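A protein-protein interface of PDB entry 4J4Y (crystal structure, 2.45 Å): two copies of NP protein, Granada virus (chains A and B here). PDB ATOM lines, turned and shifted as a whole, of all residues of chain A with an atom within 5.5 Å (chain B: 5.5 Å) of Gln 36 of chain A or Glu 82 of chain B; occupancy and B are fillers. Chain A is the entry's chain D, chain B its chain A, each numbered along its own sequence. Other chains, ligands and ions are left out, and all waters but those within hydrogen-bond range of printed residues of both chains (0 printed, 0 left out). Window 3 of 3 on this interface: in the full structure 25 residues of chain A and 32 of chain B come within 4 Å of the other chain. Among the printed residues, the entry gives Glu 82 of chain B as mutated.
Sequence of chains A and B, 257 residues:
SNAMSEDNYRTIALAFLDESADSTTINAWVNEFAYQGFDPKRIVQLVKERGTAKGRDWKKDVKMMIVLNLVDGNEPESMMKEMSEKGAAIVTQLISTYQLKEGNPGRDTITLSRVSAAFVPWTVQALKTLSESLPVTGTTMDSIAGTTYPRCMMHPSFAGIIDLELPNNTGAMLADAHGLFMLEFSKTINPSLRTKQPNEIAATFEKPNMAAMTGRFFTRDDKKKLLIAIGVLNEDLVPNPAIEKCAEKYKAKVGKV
The backbone carbonyl oxygen of Glu 82 of chain B lies close to the side-chain amide oxygen of Gln 36 of chain A, 3.2 Å away.
OE1 of Glu 82 of chain B sits at hydrogen-bond distance from ND2 of Asn 104 of chain A, 2.7 Å away.
The side-chain hydroxyl of Ser 84 of chain B is in hydrogen-bond range of the backbone carbonyl oxygen of Glu 32 of chain A, at 3.2 Å.
NE2 of Gln 36 of chain A lies within hydrogen-bond range of O of Ala 34 of chain A (3.2 Å).
O of Pro 105 of chain A sits close to OE1 of Gln 36 of chain A, at 3.0 Å.
Among the printed residues, pairs that only touch across the chains: Tyr 35 of chain A with Glu 82 of chain B (3.1 Å), Phe 33 of chain A with Met 83 of chain B (3.4 Å), Gln 36 of chain A with Ser 84 of chain B (3.5 Å), Asn 104 of chain A with Lys 81 of chain B (3.7 Å), Gln 36 of chain A with Met 83 of chain B (3.9 Å) and Glu 32 of chain A with Met 83 of chain B (3.9 Å).
Of the printed residues of chain B, Phe 33 of chain A touches Met 83.
Gln 36 of chain A touches three residues of chain B.
Ser 78 of chain B touches none of the printed residues of chain A.
Met 79 of chain B touches none of the printed residues of chain A.
Printed residues of chain A within 4 Å of Lys 81 of chain B: Asn 104 (3.7 Å).
Glu 82 of chain B touches just these residues of chain A: Tyr 35, Gln 36 and Asn 104.
Printed residues of chain A within 4 Å of Ser 84 of chain B: Glu 32 and Gln 36.
The nearest printed residue of chain B that does not touch Tyr 35 of chain A is Met 83 of chain B (4.7 Å).
Of the 14 printed residues of chain A, 5 touch a printed residue of chain B.
Hydrophobic or aromatic side chains of chain A within 4 Å of the printed part of chain B: Tyr 35.
Of the 7 printed residues of chain B, 4 touch a printed residue of chain A.
Hydrophobic or aromatic side chains of chain B within 4 Å of the printed part of chain A: Met 83.
Along chain B the printed residues that touch a printed residue of chain A span positions 81 to 84.
Among the printed residues, 9 pairs touch across the chains.
No position is printed for both chains.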
ATOM      1  N   ASN A  31     -20.210  13.016 -24.913  1.00  0.00           N
ATOM      2  CA  ASN A  31     -19.763  11.772 -24.356  1.00  0.00           C
ATOM      3  C   ASN A  31     -20.689  11.309 -23.256  1.00  0.00           C
ATOM      4  O   ASN A  31     -21.084  10.179 -23.233  1.00  0.00           O
ATOM      5  CB  ASN A  31     -18.328  11.899 -23.879  1.00  0.00           C
ATOM      6  CG  ASN A  31     -17.340  11.873 -25.023  1.00  0.00           C
ATOM      7  OD1 ASN A  31     -17.644  11.382 -26.099  1.00  0.00           O
ATOM      8  ND2 ASN A  31     -16.157  12.402 -24.795  1.00  0.00           N
ATOM      9  N   GLU A  32     -21.030  12.227 -22.372  1.00  0.00           N
ATOM     10  CA  GLU A  32     -22.037  12.075 -21.324  1.00  0.00           C
ATOM     11  C   GLU A  32     -23.510  11.886 -21.765  1.00  0.00           C
ATOM     12  O   GLU A  32     -24.282  11.307 -21.056  1.00  0.00           O
ATOM     13  CB  GLU A  32     -21.897  13.192 -20.289  1.00  0.00           C
ATOM     14  CG  GLU A  32     -20.950  12.892 -19.139  1.00  0.00           C
ATOM     15  CD  GLU A  32     -19.957  14.012 -18.835  1.00  0.00           C
ATOM     16  OE1 GLU A  32     -20.371  15.143 -18.516  1.00  0.00           O
ATOM     17  OE2 GLU A  32     -18.735  13.774 -18.892  1.00  0.00           O
ATOM     18  N   PHE A  33     -23.902  12.437 -22.902  1.00  0.00           N
ATOM     19  CA  PHE A  33     -25.273  12.320 -23.378  1.00  0.00           C
ATOM     20  C   PHE A  33     -25.468  11.192 -24.348  1.00  0.00           C
ATOM     21  O   PHE A  33     -26.571  10.793 -24.631  1.00  0.00           O
ATOM     22  CB  PHE A  33     -25.688  13.565 -24.149  1.00  0.00           C
ATOM     23  CG  PHE A  33     -25.877  14.781 -23.317  1.00  0.00           C
ATOM     24  CD1 PHE A  33     -26.049  14.696 -21.965  1.00  0.00           C
ATOM     25  CD2 PHE A  33     -25.891  16.014 -23.908  1.00  0.00           C
ATOM     26  CE1 PHE A  33     -26.208  15.818 -21.214  1.00  0.00           C
ATOM     27  CE2 PHE A  33     -26.052  17.145 -23.167  1.00  0.00           C
ATOM     28  CZ  PHE A  33     -26.214  17.052 -21.817  1.00  0.00           C
ATOM     29  N   ALA A  34     -24.384  10.747 -24.933  1.00  0.00           N
ATOM     30  CA  ALA A  34     -24.419   9.705 -25.927  1.00  0.00           C
ATOM     31  C   ALA A  34     -24.718   8.359 -25.341  1.00  0.00           C
ATOM     32  O   ALA A  34     -24.268   8.050 -24.259  1.00  0.00           O
ATOM     33  CB  ALA A  34     -23.084   9.654 -26.627  1.00  0.00           C
ATOM     34  N   TYR A  35     -25.470   7.552 -26.062  1.00  0.00           N
ATOM     35  CA  TYR A  35     -25.573   6.183 -25.681  1.00  0.00           C
ATOM     36  C   TYR A  35     -24.240   5.627 -25.981  1.00  0.00           C
ATOM     37  O   TYR A  35     -23.720   5.810 -27.044  1.00  0.00           O
ATOM     38  CB  TYR A  35     -26.604   5.446 -26.502  1.00  0.00           C
ATOM     39  CG  TYR A  35     -26.511   3.958 -26.357  1.00  0.00           C
ATOM     40  CD1 TYR A  35     -26.370   3.382 -25.117  1.00  0.00           C
ATOM     41  CD2 TYR A  35     -26.489   3.139 -27.463  1.00  0.00           C
ATOM     42  CE1 TYR A  35     -26.262   2.018 -24.981  1.00  0.00           C
ATOM     43  CE2 TYR A  35     -26.373   1.782 -27.339  1.00  0.00           C
ATOM     44  CZ  TYR A  35     -26.257   1.224 -26.097  1.00  0.00           C
ATOM     45  OH  TYR A  35     -26.152  -0.141 -25.976  1.00  0.00           O
ATOM     46  N   GLN A  36     -23.728   4.856 -25.060  1.00  0.00           N
ATOM     47  CA  GLN A  36     -22.462   4.237 -25.250  1.00  0.00           C
ATOM     48  C   GLN A  36     -22.710   2.755 -25.316  1.00  0.00           C
ATOM     49  O   GLN A  36     -23.642   2.238 -24.736  1.00  0.00           O
ATOM     50  CB  GLN A  36     -21.546   4.574 -24.095  1.00  0.00           C
ATOM     51  CG  GLN A  36     -22.174   4.304 -22.754  1.00  0.00           C
ATOM     52  CD  GLN A  36     -23.238   5.302 -22.414  1.00  0.00           C
ATOM     53  OE1 GLN A  36     -24.410   5.053 -22.617  1.00  0.00           O
ATOM     54  NE2 GLN A  36     -22.827   6.442 -21.902  1.00  0.00           N
ATOM     55  N   GLY A  37     -21.856   2.072 -26.029  1.00  0.00           N
ATOM     56  CA  GLY A  37     -22.031   0.665 -26.220  1.00  0.00           C
ATOM     57  C   GLY A  37     -21.417   0.010 -25.034  1.00  0.00           C
ATOM     58  O   GLY A  37     -21.316   0.604 -23.996  1.00  0.00           O
ATOM     59  N   PHE A  38     -21.002  -1.222 -25.202  1.00  0.00           N
ATOM     60  CA  PHE A  38     -20.242  -1.881 -24.191  1.00  0.00           C
ATOM     61  C   PHE A  38     -19.307  -2.754 -24.956  1.00  0.00           C
ATOM     62  O   PHE A  38     -19.510  -2.974 -26.117  1.00  0.00           O
ATOM     63  CB  PHE A  38     -21.140  -2.712 -23.320  1.00  0.00           C
ATOM     64  CG  PHE A  38     -21.906  -3.711 -24.072  1.00  0.00           C
ATOM     65  CD1 PHE A  38     -22.808  -3.316 -24.995  1.00  0.00           C
ATOM     66  CD2 PHE A  38     -21.687  -5.039 -23.875  1.00  0.00           C
ATOM     67  CE1 PHE A  38     -23.508  -4.227 -25.708  1.00  0.00           C
ATOM     68  CE2 PHE A  38     -22.377  -5.960 -24.587  1.00  0.00           C
ATOM     69  CZ  PHE A  38     -23.293  -5.550 -25.504  1.00  0.00           C
ATOM     70  N   GLY A 103     -30.474  -0.720 -17.976  1.00  0.00           N
ATOM     71  CA  GLY A 103     -30.790  -1.111 -19.317  1.00  0.00           C
ATOM     72  C   GLY A 103     -29.571  -0.904 -20.167  1.00  0.00           C
ATOM     73  O   GLY A 103     -28.852  -1.833 -20.463  1.00  0.00           O
ATOM     74  N   ASN A 104     -29.336   0.335 -20.556  1.00  0.00           N
ATOM     75  CA  ASN A 104     -28.205   0.660 -21.375  1.00  0.00           C
ATOM     76  C   ASN A 104     -27.429   1.776 -20.738  1.00  0.00           C
ATOM     77  O   ASN A 104     -27.264   2.834 -21.328  1.00  0.00           O
ATOM     78  CB  ASN A 104     -28.691   1.034 -22.756  1.00  0.00           C
ATOM     79  CG  ASN A 104     -29.484  -0.077 -23.394  1.00  0.00           C
ATOM     80  OD1 ASN A 104     -29.546  -1.179 -22.858  1.00  0.00           O
ATOM     81  ND2 ASN A 104     -30.102   0.201 -24.531  1.00  0.00           N
ATOM     82  N   PRO A 105     -26.910   1.488 -19.466  1.00  0.00           N
ATOM     83  CA  PRO A 105     -26.394   2.680 -18.781  1.00  0.00           C
ATOM     84  C   PRO A 105     -25.040   3.013 -19.296  1.00  0.00           C
ATOM     85  O   PRO A 105     -24.864   3.043 -20.485  1.00  0.00           O
ATOM     86  CB  PRO A 105     -26.292   2.275 -17.317  1.00  0.00           C
ATOM     87  CG  PRO A 105     -26.756   0.881 -17.221  1.00  0.00           C
ATOM     88  CD  PRO A 105     -26.566   0.298 -18.557  1.00  0.00           C
ATOM     89  N   GLY A 106     -24.096   3.263 -18.413  1.00  0.00           N
ATOM     90  CA  GLY A 106     -22.749   3.519 -18.846  1.00  0.00           C
ATOM     91  C   GLY A 106     -21.976   2.259 -19.100  1.00  0.00           C
ATOM     92  O   GLY A 106     -22.396   1.182 -18.727  1.00  0.00           O
ATOM     93  N   ARG A 107     -20.814   2.421 -19.704  1.00  0.00           N
ATOM     94  CA  ARG A 107     -19.938   1.321 -20.001  1.00  0.00           C
ATOM     95  C   ARG A 107     -19.457   0.729 -18.700  1.00  0.00           C
ATOM     96  O   ARG A 107     -19.440   1.385 -17.690  1.00  0.00           O
ATOM     97  CB  ARG A 107     -18.714   1.803 -20.784  1.00  0.00           C
ATOM     98  CG  ARG A 107     -18.928   2.074 -22.250  1.00  0.00           C
ATOM     99  CD  ARG A 107     -17.651   1.860 -23.035  1.00  0.00           C
ATOM    100  NE  ARG A 107     -17.926   1.734 -24.459  1.00  0.00           N
ATOM    101  CZ  ARG A 107     -17.239   0.970 -25.290  1.00  0.00           C
ATOM    102  NH1 ARG A 107     -16.219   0.270 -24.845  1.00  0.00           N
ATOM    103  NH2 ARG A 107     -17.572   0.916 -26.561  1.00  0.00           N
ATOM    104  N   ARG A 114     -26.915  -7.766 -21.736  1.00  0.00           N
ATOM    105  CA  ARG A 114     -25.511  -7.700 -22.027  1.00  0.00           C
ATOM    106  C   ARG A 114     -24.839  -9.031 -21.892  1.00  0.00           C
ATOM    107  O   ARG A 114     -24.030  -9.412 -22.681  1.00  0.00           O
ATOM    108  CB  ARG A 114     -24.849  -6.637 -21.160  1.00  0.00           C
ATOM    109  CG  ARG A 114     -24.654  -5.340 -21.904  1.00  0.00           C
ATOM    110  CD  ARG A 114     -24.440  -4.127 -21.040  1.00  0.00           C
ATOM    111  NE  ARG A 114     -24.886  -2.931 -21.745  1.00  0.00           N
ATOM    112  CZ  ARG A 114     -24.360  -1.722 -21.600  1.00  0.00           C
ATOM    113  NH1 ARG A 114     -23.364  -1.525 -20.760  1.00  0.00           N
ATOM    114  NH2 ARG A 114     -24.833  -0.711 -22.295  1.00  0.00           N
ATOM    115  N   SER B  78     -37.603  10.349 -22.829  1.00  0.00           N
ATOM    116  CA  SER B  78     -37.411   9.098 -23.503  1.00  0.00           C
ATOM    117  C   SER B  78     -35.975   8.907 -23.889  1.00  0.00           C
ATOM    118  O   SER B  78     -35.606   7.859 -24.354  1.00  0.00           O
ATOM    119  CB  SER B  78     -38.303   9.005 -24.714  1.00  0.00           C
ATOM    120  OG  SER B  78     -37.904   7.930 -25.503  1.00  0.00           O
ATOM    121  N   MET B  79     -35.193   9.957 -23.798  1.00  0.00           N
ATOM    122  CA  MET B  79     -33.774   9.851 -24.024  1.00  0.00           C
ATOM    123  C   MET B  79     -33.075   9.079 -22.940  1.00  0.00           C
ATOM    124  O   MET B  79     -32.237   8.240 -23.198  1.00  0.00           O
ATOM    125  CB  MET B  79     -33.153  11.234 -24.109  1.00  0.00           C
ATOM    126  CG  MET B  79     -33.867  12.191 -25.026  1.00  0.00           C
ATOM    127  SD  MET B  79     -33.163  13.836 -25.010  1.00  0.00           S
ATOM    128  CE  MET B  79     -34.318  14.603 -26.108  1.00  0.00           C
ATOM    129  N   MET B  80     -33.445   9.378 -21.707  1.00  0.00           N
ATOM    130  CA  MET B  80     -32.590   9.275 -20.543  1.00  0.00           C
ATOM    131  C   MET B  80     -32.123   7.861 -20.302  1.00  0.00           C
ATOM    132  O   MET B  80     -31.134   7.627 -19.663  1.00  0.00           O
ATOM    133  CB  MET B  80     -33.323   9.751 -19.299  1.00  0.00           C
ATOM    134  CG  MET B  80     -34.006  11.099 -19.377  1.00  0.00           C
ATOM    135  SD  MET B  80     -34.100  11.892 -17.766  1.00  0.00           S
ATOM    136  CE  MET B  80     -32.379  11.909 -17.303  1.00  0.00           C
ATOM    137  N   LYS B  81     -32.862   6.918 -20.842  1.00  0.00           N
ATOM    138  CA  LYS B  81     -32.640   5.521 -20.591  1.00  0.00           C
ATOM    139  C   LYS B  81     -31.258   5.097 -21.056  1.00  0.00           C
ATOM    140  O   LYS B  81     -30.612   4.268 -20.442  1.00  0.00           O
ATOM    141  CB  LYS B  81     -33.714   4.717 -21.315  1.00  0.00           C
ATOM    142  CG  LYS B  81     -33.479   3.220 -21.292  1.00  0.00           C
ATOM    143  CD  LYS B  81     -34.684   2.420 -21.760  1.00  0.00           C
ATOM    144  CE  LYS B  81     -35.154   1.475 -20.673  1.00  0.00           C
ATOM    145  NZ  LYS B  81     -36.621   1.241 -20.734  1.00  0.00           N
ATOM    146  N   GLU B  82     -30.819   5.679 -22.157  1.00  0.00           N
ATOM    147  CA  GLU B  82     -29.669   5.184 -22.853  1.00  0.00           C
ATOM    148  C   GLU B  82     -28.398   5.923 -22.637  1.00  0.00           C
ATOM    149  O   GLU B  82     -27.452   5.647 -23.310  1.00  0.00           O
ATOM    150  CB  GLU B  82     -29.943   5.105 -24.343  1.00  0.00           C
ATOM    151  CG  GLU B  82     -30.173   3.695 -24.823  1.00  0.00           C
ATOM    152  CD  GLU B  82     -31.586   3.230 -24.583  1.00  0.00           C
ATOM    153  OE1 GLU B  82     -31.773   2.242 -23.854  1.00  0.00           O
ATOM    154  OE2 GLU B  82     -32.517   3.856 -25.116  1.00  0.00           O
ATOM    155  N   MET B  83     -28.349   6.829 -21.698  1.00  0.00           N
ATOM    156  CA  MET B  83     -27.135   7.577 -21.502  1.00  0.00           C
ATOM    157  C   MET B  83     -26.592   7.392 -20.118  1.00  0.00           C
ATOM    158  O   MET B  83     -27.247   6.881 -19.250  1.00  0.00           O
ATOM    159  CB  MET B  83     -27.350   9.047 -21.814  1.00  0.00           C
ATOM    160  CG  MET B  83     -27.883   9.871 -20.671  1.00  0.00           C
ATOM    161  SD  MET B  83     -28.626  11.369 -21.233  1.00  0.00           S
ATOM    162  CE  MET B  83     -30.191  10.753 -21.798  1.00  0.00           C
ATOM    163  N   SER B  84     -25.386   7.853 -19.923  1.00  0.00           N
ATOM    164  CA  SER B  84     -24.742   7.680 -18.660  1.00  0.00           C
ATOM    165  C   SER B  84     -25.451   8.489 -17.644  1.00  0.00           C
ATOM    166  O   SER B  84     -26.140   9.407 -17.942  1.00  0.00           O
ATOM    167  CB  SER B  84     -23.285   8.063 -18.729  1.00  0.00           C
ATOM    168  OG  SER B  84     -23.131   9.439 -18.705  1.00  0.00           O
